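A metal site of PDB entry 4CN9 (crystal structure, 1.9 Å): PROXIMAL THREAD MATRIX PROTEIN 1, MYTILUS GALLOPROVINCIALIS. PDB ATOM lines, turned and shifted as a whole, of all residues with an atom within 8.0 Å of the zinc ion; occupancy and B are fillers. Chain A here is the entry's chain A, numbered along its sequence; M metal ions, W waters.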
ATOM      1  N   ASP A  61     -20.078  14.318   7.924  1.00  0.00           N
ATOM      2  CA  ASP A  61     -19.880  13.480   9.123  1.00  0.00           C
ATOM      3  C   ASP A  61     -19.762  14.386  10.359  1.00  0.00           C
ATOM      4  O   ASP A  61     -18.877  15.257  10.384  1.00  0.00           O
ATOM      5  CB  ASP A  61     -18.616  12.647   8.918  1.00  0.00           C
ATOM      6  CG  ASP A  61     -18.310  11.641  10.053  1.00  0.00           C
ATOM      7  OD1 ASP A  61     -18.593  11.899  11.242  1.00  0.00           O
ATOM      8  OD2 ASP A  61     -17.723  10.594   9.728  1.00  0.00           O
ATOM      9  N   ASP A  62     -20.659  14.240  11.341  1.00  0.00           N
ATOM     10  CA  ASP A  62     -20.504  14.991  12.604  1.00  0.00           C
ATOM     11  C   ASP A  62     -20.325  14.075  13.815  1.00  0.00           C
ATOM     12  O   ASP A  62     -20.800  14.367  14.903  1.00  0.00           O
ATOM     13  CB  ASP A  62     -21.598  16.068  12.818  1.00  0.00           C
ATOM     14  CG  ASP A  62     -23.011  15.505  13.012  1.00  0.00           C
ATOM     15  OD1 ASP A  62     -23.261  14.290  12.816  1.00  0.00           O
ATOM     16  OD2 ASP A  62     -23.898  16.310  13.374  1.00  0.00           O
ATOM     17  N   SER A  63     -19.585  12.984  13.606  1.00  0.00           N
ATOM     18  CA  SER A  63     -19.227  12.056  14.686  1.00  0.00           C
ATOM     19  C   SER A  63     -18.211  12.659  15.656  1.00  0.00           C
ATOM     20  O   SER A  63     -17.394  13.505  15.282  1.00  0.00           O
ATOM     21  CB  SER A  63     -18.664  10.744  14.107  1.00  0.00           C
ATOM     22  OG  SER A  63     -17.435  10.935  13.401  1.00  0.00           O
ATOM     23  N   SER A  64     -18.235  12.172  16.895  1.00  0.00           N
ATOM     24  CA  SER A  64     -17.395  12.709  17.970  1.00  0.00           C
ATOM     25  C   SER A  64     -15.909  12.478  17.712  1.00  0.00           C
ATOM     26  O   SER A  64     -15.078  13.228  18.210  1.00  0.00           O
ATOM     27  CB  SER A  64     -17.788  12.072  19.308  1.00  0.00           C
ATOM     28  OG  SER A  64     -17.606  10.666  19.254  1.00  0.00           O
ATOM     29  N   SER A  65     -15.573  11.464  16.932  1.00  0.00           N
ATOM     30  CA  SER A  65     -14.171  11.200  16.566  1.00  0.00           C
ATOM     31  C   SER A  65     -13.457  12.438  16.010  1.00  0.00           C
ATOM     32  O   SER A  65     -12.263  12.628  16.247  1.00  0.00           O
ATOM     33  CB  SER A  65     -14.115  10.080  15.519  1.00  0.00           C
ATOM     34  OG  SER A  65     -14.684  10.522  14.291  1.00  0.00           O
ATOM     35  N   ILE A  66     -14.191  13.280  15.303  1.00  0.00           N
ATOM     36  CA  ILE A  66     -13.623  14.447  14.661  1.00  0.00           C
ATOM     37  C   ILE A  66     -13.198  15.494  15.674  1.00  0.00           C
ATOM     38  O   ILE A  66     -12.131  16.097  15.539  1.00  0.00           O
ATOM     39  CB  ILE A  66     -14.630  15.066  13.672  1.00  0.00           C
ATOM     40  CG1 ILE A  66     -14.957  14.036  12.589  1.00  0.00           C
ATOM     41  CG2 ILE A  66     -14.067  16.371  13.075  1.00  0.00           C
ATOM     42  CD1 ILE A  66     -16.033  14.447  11.628  1.00  0.00           C
ATOM     43  N   GLN A  67     -14.040  15.711  16.686  1.00  0.00           N
ATOM     44  CA  GLN A  67     -13.775  16.706  17.704  1.00  0.00           C
ATOM     45  C   GLN A  67     -12.650  16.222  18.623  1.00  0.00           C
ATOM     46  O   GLN A  67     -11.790  17.006  18.999  1.00  0.00           O
ATOM     47  CB  GLN A  67     -15.063  17.019  18.492  1.00  0.00           C
ATOM     48  CG  GLN A  67     -14.897  18.012  19.652  1.00  0.00           C
ATOM     49  CD  GLN A  67     -14.567  19.421  19.186  1.00  0.00           C
ATOM     50  OE1 GLN A  67     -14.934  19.846  18.089  1.00  0.00           O
ATOM     51  NE2 GLN A  67     -13.867  20.162  20.047  1.00  0.00           N
ATOM     52  N   TYR A  74     -13.614  20.697  12.601  1.00  0.00           N
ATOM     53  CA  TYR A  74     -14.908  21.085  12.035  1.00  0.00           C
ATOM     54  C   TYR A  74     -14.813  22.387  11.250  1.00  0.00           C
ATOM     55  O   TYR A  74     -15.463  22.542  10.219  1.00  0.00           O
ATOM     56  CB  TYR A  74     -15.989  21.222  13.114  1.00  0.00           C
ATOM     57  CG  TYR A  74     -16.576  19.906  13.566  1.00  0.00           C
ATOM     58  CD1 TYR A  74     -17.057  18.971  12.639  1.00  0.00           C
ATOM     59  CD2 TYR A  74     -16.653  19.594  14.924  1.00  0.00           C
ATOM     60  CE1 TYR A  74     -17.600  17.767  13.066  1.00  0.00           C
ATOM     61  CE2 TYR A  74     -17.189  18.377  15.349  1.00  0.00           C
ATOM     62  CZ  TYR A  74     -17.659  17.466  14.411  1.00  0.00           C
ATOM     63  OH  TYR A  74     -18.208  16.268  14.827  1.00  0.00           O
ATOM     64  N   PHE A 106     -24.568  13.823   9.467  1.00  0.00           N
ATOM     65  CA  PHE A 106     -24.841  12.438   9.816  1.00  0.00           C
ATOM     66  C   PHE A 106     -23.781  11.874  10.753  1.00  0.00           C
ATOM     67  O   PHE A 106     -22.580  12.170  10.605  1.00  0.00           O
ATOM     68  CB  PHE A 106     -24.942  11.562   8.552  1.00  0.00           C
ATOM     69  CG  PHE A 106     -23.597  11.116   8.016  1.00  0.00           C
ATOM     70  CD1 PHE A 106     -22.869  11.938   7.147  1.00  0.00           C
ATOM     71  CD2 PHE A 106     -23.046   9.910   8.403  1.00  0.00           C
ATOM     72  CE1 PHE A 106     -21.620  11.542   6.683  1.00  0.00           C
ATOM     73  CE2 PHE A 106     -21.791   9.508   7.950  1.00  0.00           C
ATOM     74  CZ  PHE A 106     -21.087  10.324   7.082  1.00  0.00           C
ATOM     75  N   SER A 107     -24.235  11.102  11.735  1.00  0.00           N
ATOM     76  CA  SER A 107     -23.369  10.253  12.563  1.00  0.00           C
ATOM     77  C   SER A 107     -24.290   9.283  13.293  1.00  0.00           C
ATOM     78  O   SER A 107     -24.573   8.181  12.800  1.00  0.00           O
ATOM     79  CB  SER A 107     -22.466  11.055  13.527  1.00  0.00           C
ATOM     80  OG  SER A 107     -23.149  12.046  14.278  1.00  0.00           O
ATOM     81  N   GLY A 137     -22.004  12.716  17.272  1.00  0.00           N
ATOM     82  CA  GLY A 137     -22.652  11.433  17.525  1.00  0.00           C
ATOM     83  C   GLY A 137     -21.659  10.324  17.788  1.00  0.00           C
ATOM     84  O   GLY A 137     -20.492  10.376  17.368  1.00  0.00           O
ATOM     85  N   GLY A 138     -22.130   9.287  18.485  1.00  0.00           N
ATOM     86  CA  GLY A 138     -21.292   8.168  18.890  1.00  0.00           C
ATOM     87  C   GLY A 138     -21.281   7.004  17.924  1.00  0.00           C
ATOM     88  O   GLY A 138     -20.735   5.952  18.238  1.00  0.00           O
ATOM     89  N   GLN A 139     -21.901   7.187  16.757  1.00  0.00           N
ATOM     90  CA  GLN A 139     -22.016   6.173  15.720  1.00  0.00           C
ATOM     91  C   GLN A 139     -21.761   6.841  14.366  1.00  0.00           C
ATOM     92  O   GLN A 139     -21.830   8.061  14.264  1.00  0.00           O
ATOM     93  CB  GLN A 139     -23.435   5.610  15.656  1.00  0.00           C
ATOM     94  CG  GLN A 139     -23.962   4.964  16.910  1.00  0.00           C
ATOM     95  CD  GLN A 139     -25.353   4.380  16.694  1.00  0.00           C
ATOM     96  OE1 GLN A 139     -26.068   4.756  15.759  1.00  0.00           O
ATOM     97  NE2 GLN A 139     -25.750   3.452  17.565  1.00  0.00           N
ATOM     98  N   THR A 140     -21.540   6.043  13.330  1.00  0.00           N
ATOM     99  CA  THR A 140     -21.399   6.565  11.965  1.00  0.00           C
ATOM    100  C   THR A 140     -22.334   5.827  11.001  1.00  0.00           C
ATOM    101  O   THR A 140     -22.025   4.730  10.539  1.00  0.00           O
ATOM    102  CB  THR A 140     -19.939   6.448  11.480  1.00  0.00           C
ATOM    103  OG1 THR A 140     -19.078   7.152  12.385  1.00  0.00           O
ATOM    104  CG2 THR A 140     -19.755   7.033  10.074  1.00  0.00           C
ATOM    105  N   THR A 173     -16.305  11.759   5.280  1.00  0.00           N
ATOM    106  CA  THR A 173     -16.323  10.974   6.510  1.00  0.00           C
ATOM    107  C   THR A 173     -14.931  10.629   7.048  1.00  0.00           C
ATOM    108  O   THR A 173     -13.971  10.543   6.287  1.00  0.00           O
ATOM    109  CB  THR A 173     -17.139   9.684   6.302  1.00  0.00           C
ATOM    110  OG1 THR A 173     -17.266   8.973   7.552  1.00  0.00           O
ATOM    111  CG2 THR A 173     -16.504   8.802   5.271  1.00  0.00           C
ATOM    112  N   ASP A 174     -14.839  10.467   8.371  1.00  0.00           N
ATOM    113  CA  ASP A 174     -13.601  10.007   8.982  1.00  0.00           C
ATOM    114  C   ASP A 174     -13.782   8.630   9.600  1.00  0.00           C
ATOM    115  O   ASP A 174     -12.975   8.199  10.426  1.00  0.00           O
ATOM    116  CB  ASP A 174     -13.114  11.010  10.035  1.00  0.00           C
ATOM    117  CG  ASP A 174     -13.794  10.837  11.395  1.00  0.00           C
ATOM    118  OD1 ASP A 174     -14.986  10.418  11.460  1.00  0.00           O
ATOM    119  OD2 ASP A 174     -13.114  11.127  12.409  1.00  0.00           O
ATOM    120  N   GLY A 175     -14.821   7.923   9.176  1.00  0.00           N
ATOM    121  CA  GLY A 175     -15.153   6.661   9.824  1.00  0.00           C
ATOM    122  C   GLY A 175     -15.701   5.598   8.897  1.00  0.00           C
ATOM    123  O   GLY A 175     -15.865   5.817   7.690  1.00  0.00           O
ATOM    124  N   LYS A 176     -15.998   4.441   9.459  1.00  0.00           N
ATOM    125  CA  LYS A 176     -16.634   3.388   8.693  1.00  0.00           C
ATOM    126  C   LYS A 176     -18.055   3.235   9.212  1.00  0.00           C
ATOM    127  O   LYS A 176     -18.317   3.507  10.379  1.00  0.00           O
ATOM    128  CB  LYS A 176     -15.863   2.073   8.809  1.00  0.00           C
ATOM    129  CG  LYS A 176     -15.868   1.455  10.188  1.00  0.00           C
ATOM    130  CD  LYS A 176     -15.165   0.104  10.168  1.00  0.00           C
ATOM    131  CE  LYS A 176     -14.799  -0.338  11.570  1.00  0.00           C
ATOM    132  NZ  LYS A 176     -14.035  -1.624  11.571  1.00  0.00           N
ATOM    133  N   ASN A 178     -21.084   1.870  10.860  1.00  0.00           N
ATOM    134  CA  ASN A 178     -21.166   0.837  11.896  1.00  0.00           C
ATOM    135  C   ASN A 178     -22.531   0.721  12.557  1.00  0.00           C
ATOM    136  O   ASN A 178     -22.649   0.123  13.615  1.00  0.00           O
ATOM    137  CB  ASN A 178     -20.097   1.037  12.970  1.00  0.00           C
ATOM    138  CG  ASN A 178     -20.251   2.363  13.719  1.00  0.00           C
ATOM    139  OD1 ASN A 178     -21.142   3.138  13.447  1.00  0.00           O
ATOM    140  ND2 ASN A 178     -19.369   2.604  14.676  1.00  0.00           N
ATOM    141  N   ILE A 202     -11.227  10.856   5.263  1.00  0.00           N
ATOM    142  CA  ILE A 202     -10.207  11.573   6.016  1.00  0.00           C
ATOM    143  C   ILE A 202      -9.674  10.728   7.164  1.00  0.00           C
ATOM    144  O   ILE A 202     -10.431  10.164   7.942  1.00  0.00           O
ATOM    145  CB  ILE A 202     -10.775  12.880   6.558  1.00  0.00           C
ATOM    146  CG1 ILE A 202     -11.309  13.725   5.411  1.00  0.00           C
ATOM    147  CG2 ILE A 202      -9.684  13.665   7.293  1.00  0.00           C
ATOM    148  CD1 ILE A 202     -12.681  14.289   5.632  1.00  0.00           C
ATOM    149  N   GLY A 205      -9.624   6.083   9.851  1.00  0.00           N
ATOM    150  CA  GLY A 205     -10.788   5.363  10.369  1.00  0.00           C
ATOM    151  C   GLY A 205     -11.818   4.900   9.341  1.00  0.00           C
ATOM    152  O   GLY A 205     -12.627   4.022   9.630  1.00  0.00           O
ATOM    153  N   PHE A 206     -11.791   5.489   8.149  1.00  0.00           N
ATOM    154  CA  PHE A 206     -12.680   5.056   7.069  1.00  0.00           C
ATOM    155  C   PHE A 206     -12.101   3.807   6.384  1.00  0.00           C
ATOM    156  O   PHE A 206     -10.913   3.516   6.524  1.00  0.00           O
ATOM    157  CB  PHE A 206     -12.877   6.206   6.054  1.00  0.00           C
ATOM    158  CG  PHE A 206     -11.688   6.428   5.144  1.00  0.00           C
ATOM    159  CD1 PHE A 206     -11.577   5.736   3.949  1.00  0.00           C
ATOM    160  CD2 PHE A 206     -10.683   7.323   5.485  1.00  0.00           C
ATOM    161  CE1 PHE A 206     -10.495   5.926   3.124  1.00  0.00           C
ATOM    162  CE2 PHE A 206      -9.587   7.522   4.657  1.00  0.00           C
ATOM    163  CZ  PHE A 206      -9.492   6.828   3.479  1.00  0.00           C
ATOM    164  N   PHE A 227      -7.476  16.592   8.229  1.00  0.00           N
ATOM    165  CA  PHE A 227      -8.417  17.644   7.887  1.00  0.00           C
ATOM    166  C   PHE A 227      -7.664  18.872   7.386  1.00  0.00           C
ATOM    167  O   PHE A 227      -8.195  19.680   6.639  1.00  0.00           O
ATOM    168  CB  PHE A 227      -9.282  17.992   9.103  1.00  0.00           C
ATOM    169  CG  PHE A 227     -10.178  16.870   9.545  1.00  0.00           C
ATOM    170  CD1 PHE A 227      -9.734  15.917  10.447  1.00  0.00           C
ATOM    171  CD2 PHE A 227     -11.461  16.747   9.044  1.00  0.00           C
ATOM    172  CE1 PHE A 227     -10.560  14.882  10.854  1.00  0.00           C
ATOM    173  CE2 PHE A 227     -12.295  15.709   9.436  1.00  0.00           C
ATOM    174  CZ  PHE A 227     -11.843  14.778  10.337  1.00  0.00           C
HETATM  175 ZN    ZN M   1     -15.915   9.428  13.080  1.00  0.00          ZN
HETATM  176  O   HOH W   1     -17.123   8.710  11.549  1.00  0.00           O
HETATM  177  O   HOH W   2     -16.737   8.208  14.550  1.00  0.00           O
HETATM  178  O   HOH W   3     -14.491   7.877  12.922  1.00  0.00           O
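Water W1 lies within hydrogen-bond range of the side-chain hydroxyl of Thr 140 (2.6 Å), the side-chain carboxylate of Asp 61 (2.7 Å) and the backbone NH of Gly 175 (3.4 Å).
The zinc ion is bound by OG of Ser 65, water W1, water W2, water W3, OD1 of Asp 174 and OG of Ser 63.
OD2 of Asp 61 touches the zinc ion (3.98 Å).
Thr 140 touches the zinc ion.
Along chain A the residues within 4 Å of the zinc ion span positions 61 to 174.
The nearest printed residue that does not touch the zinc ion is Gly 175 (4.3 Å).
OD2 of Asp 61 lies within hydrogen-bond range of N of Asp 174.
The side-chain carboxylate (OD1) of Asp 61 sits at hydrogen-bond distance from the backbone NH (N) of Ser 63, 2.8 Å away.
O of Ser 63 sits at hydrogen-bond distance from OH of Tyr 74, at 2.9 Å.
N of Thr 140 sits at hydrogen-bond distance from OD1 of Asn 178 (2.9 Å).
OD2 of Asp 61 is in hydrogen-bond range of OG1 of Thr 173 (2.8 Å).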
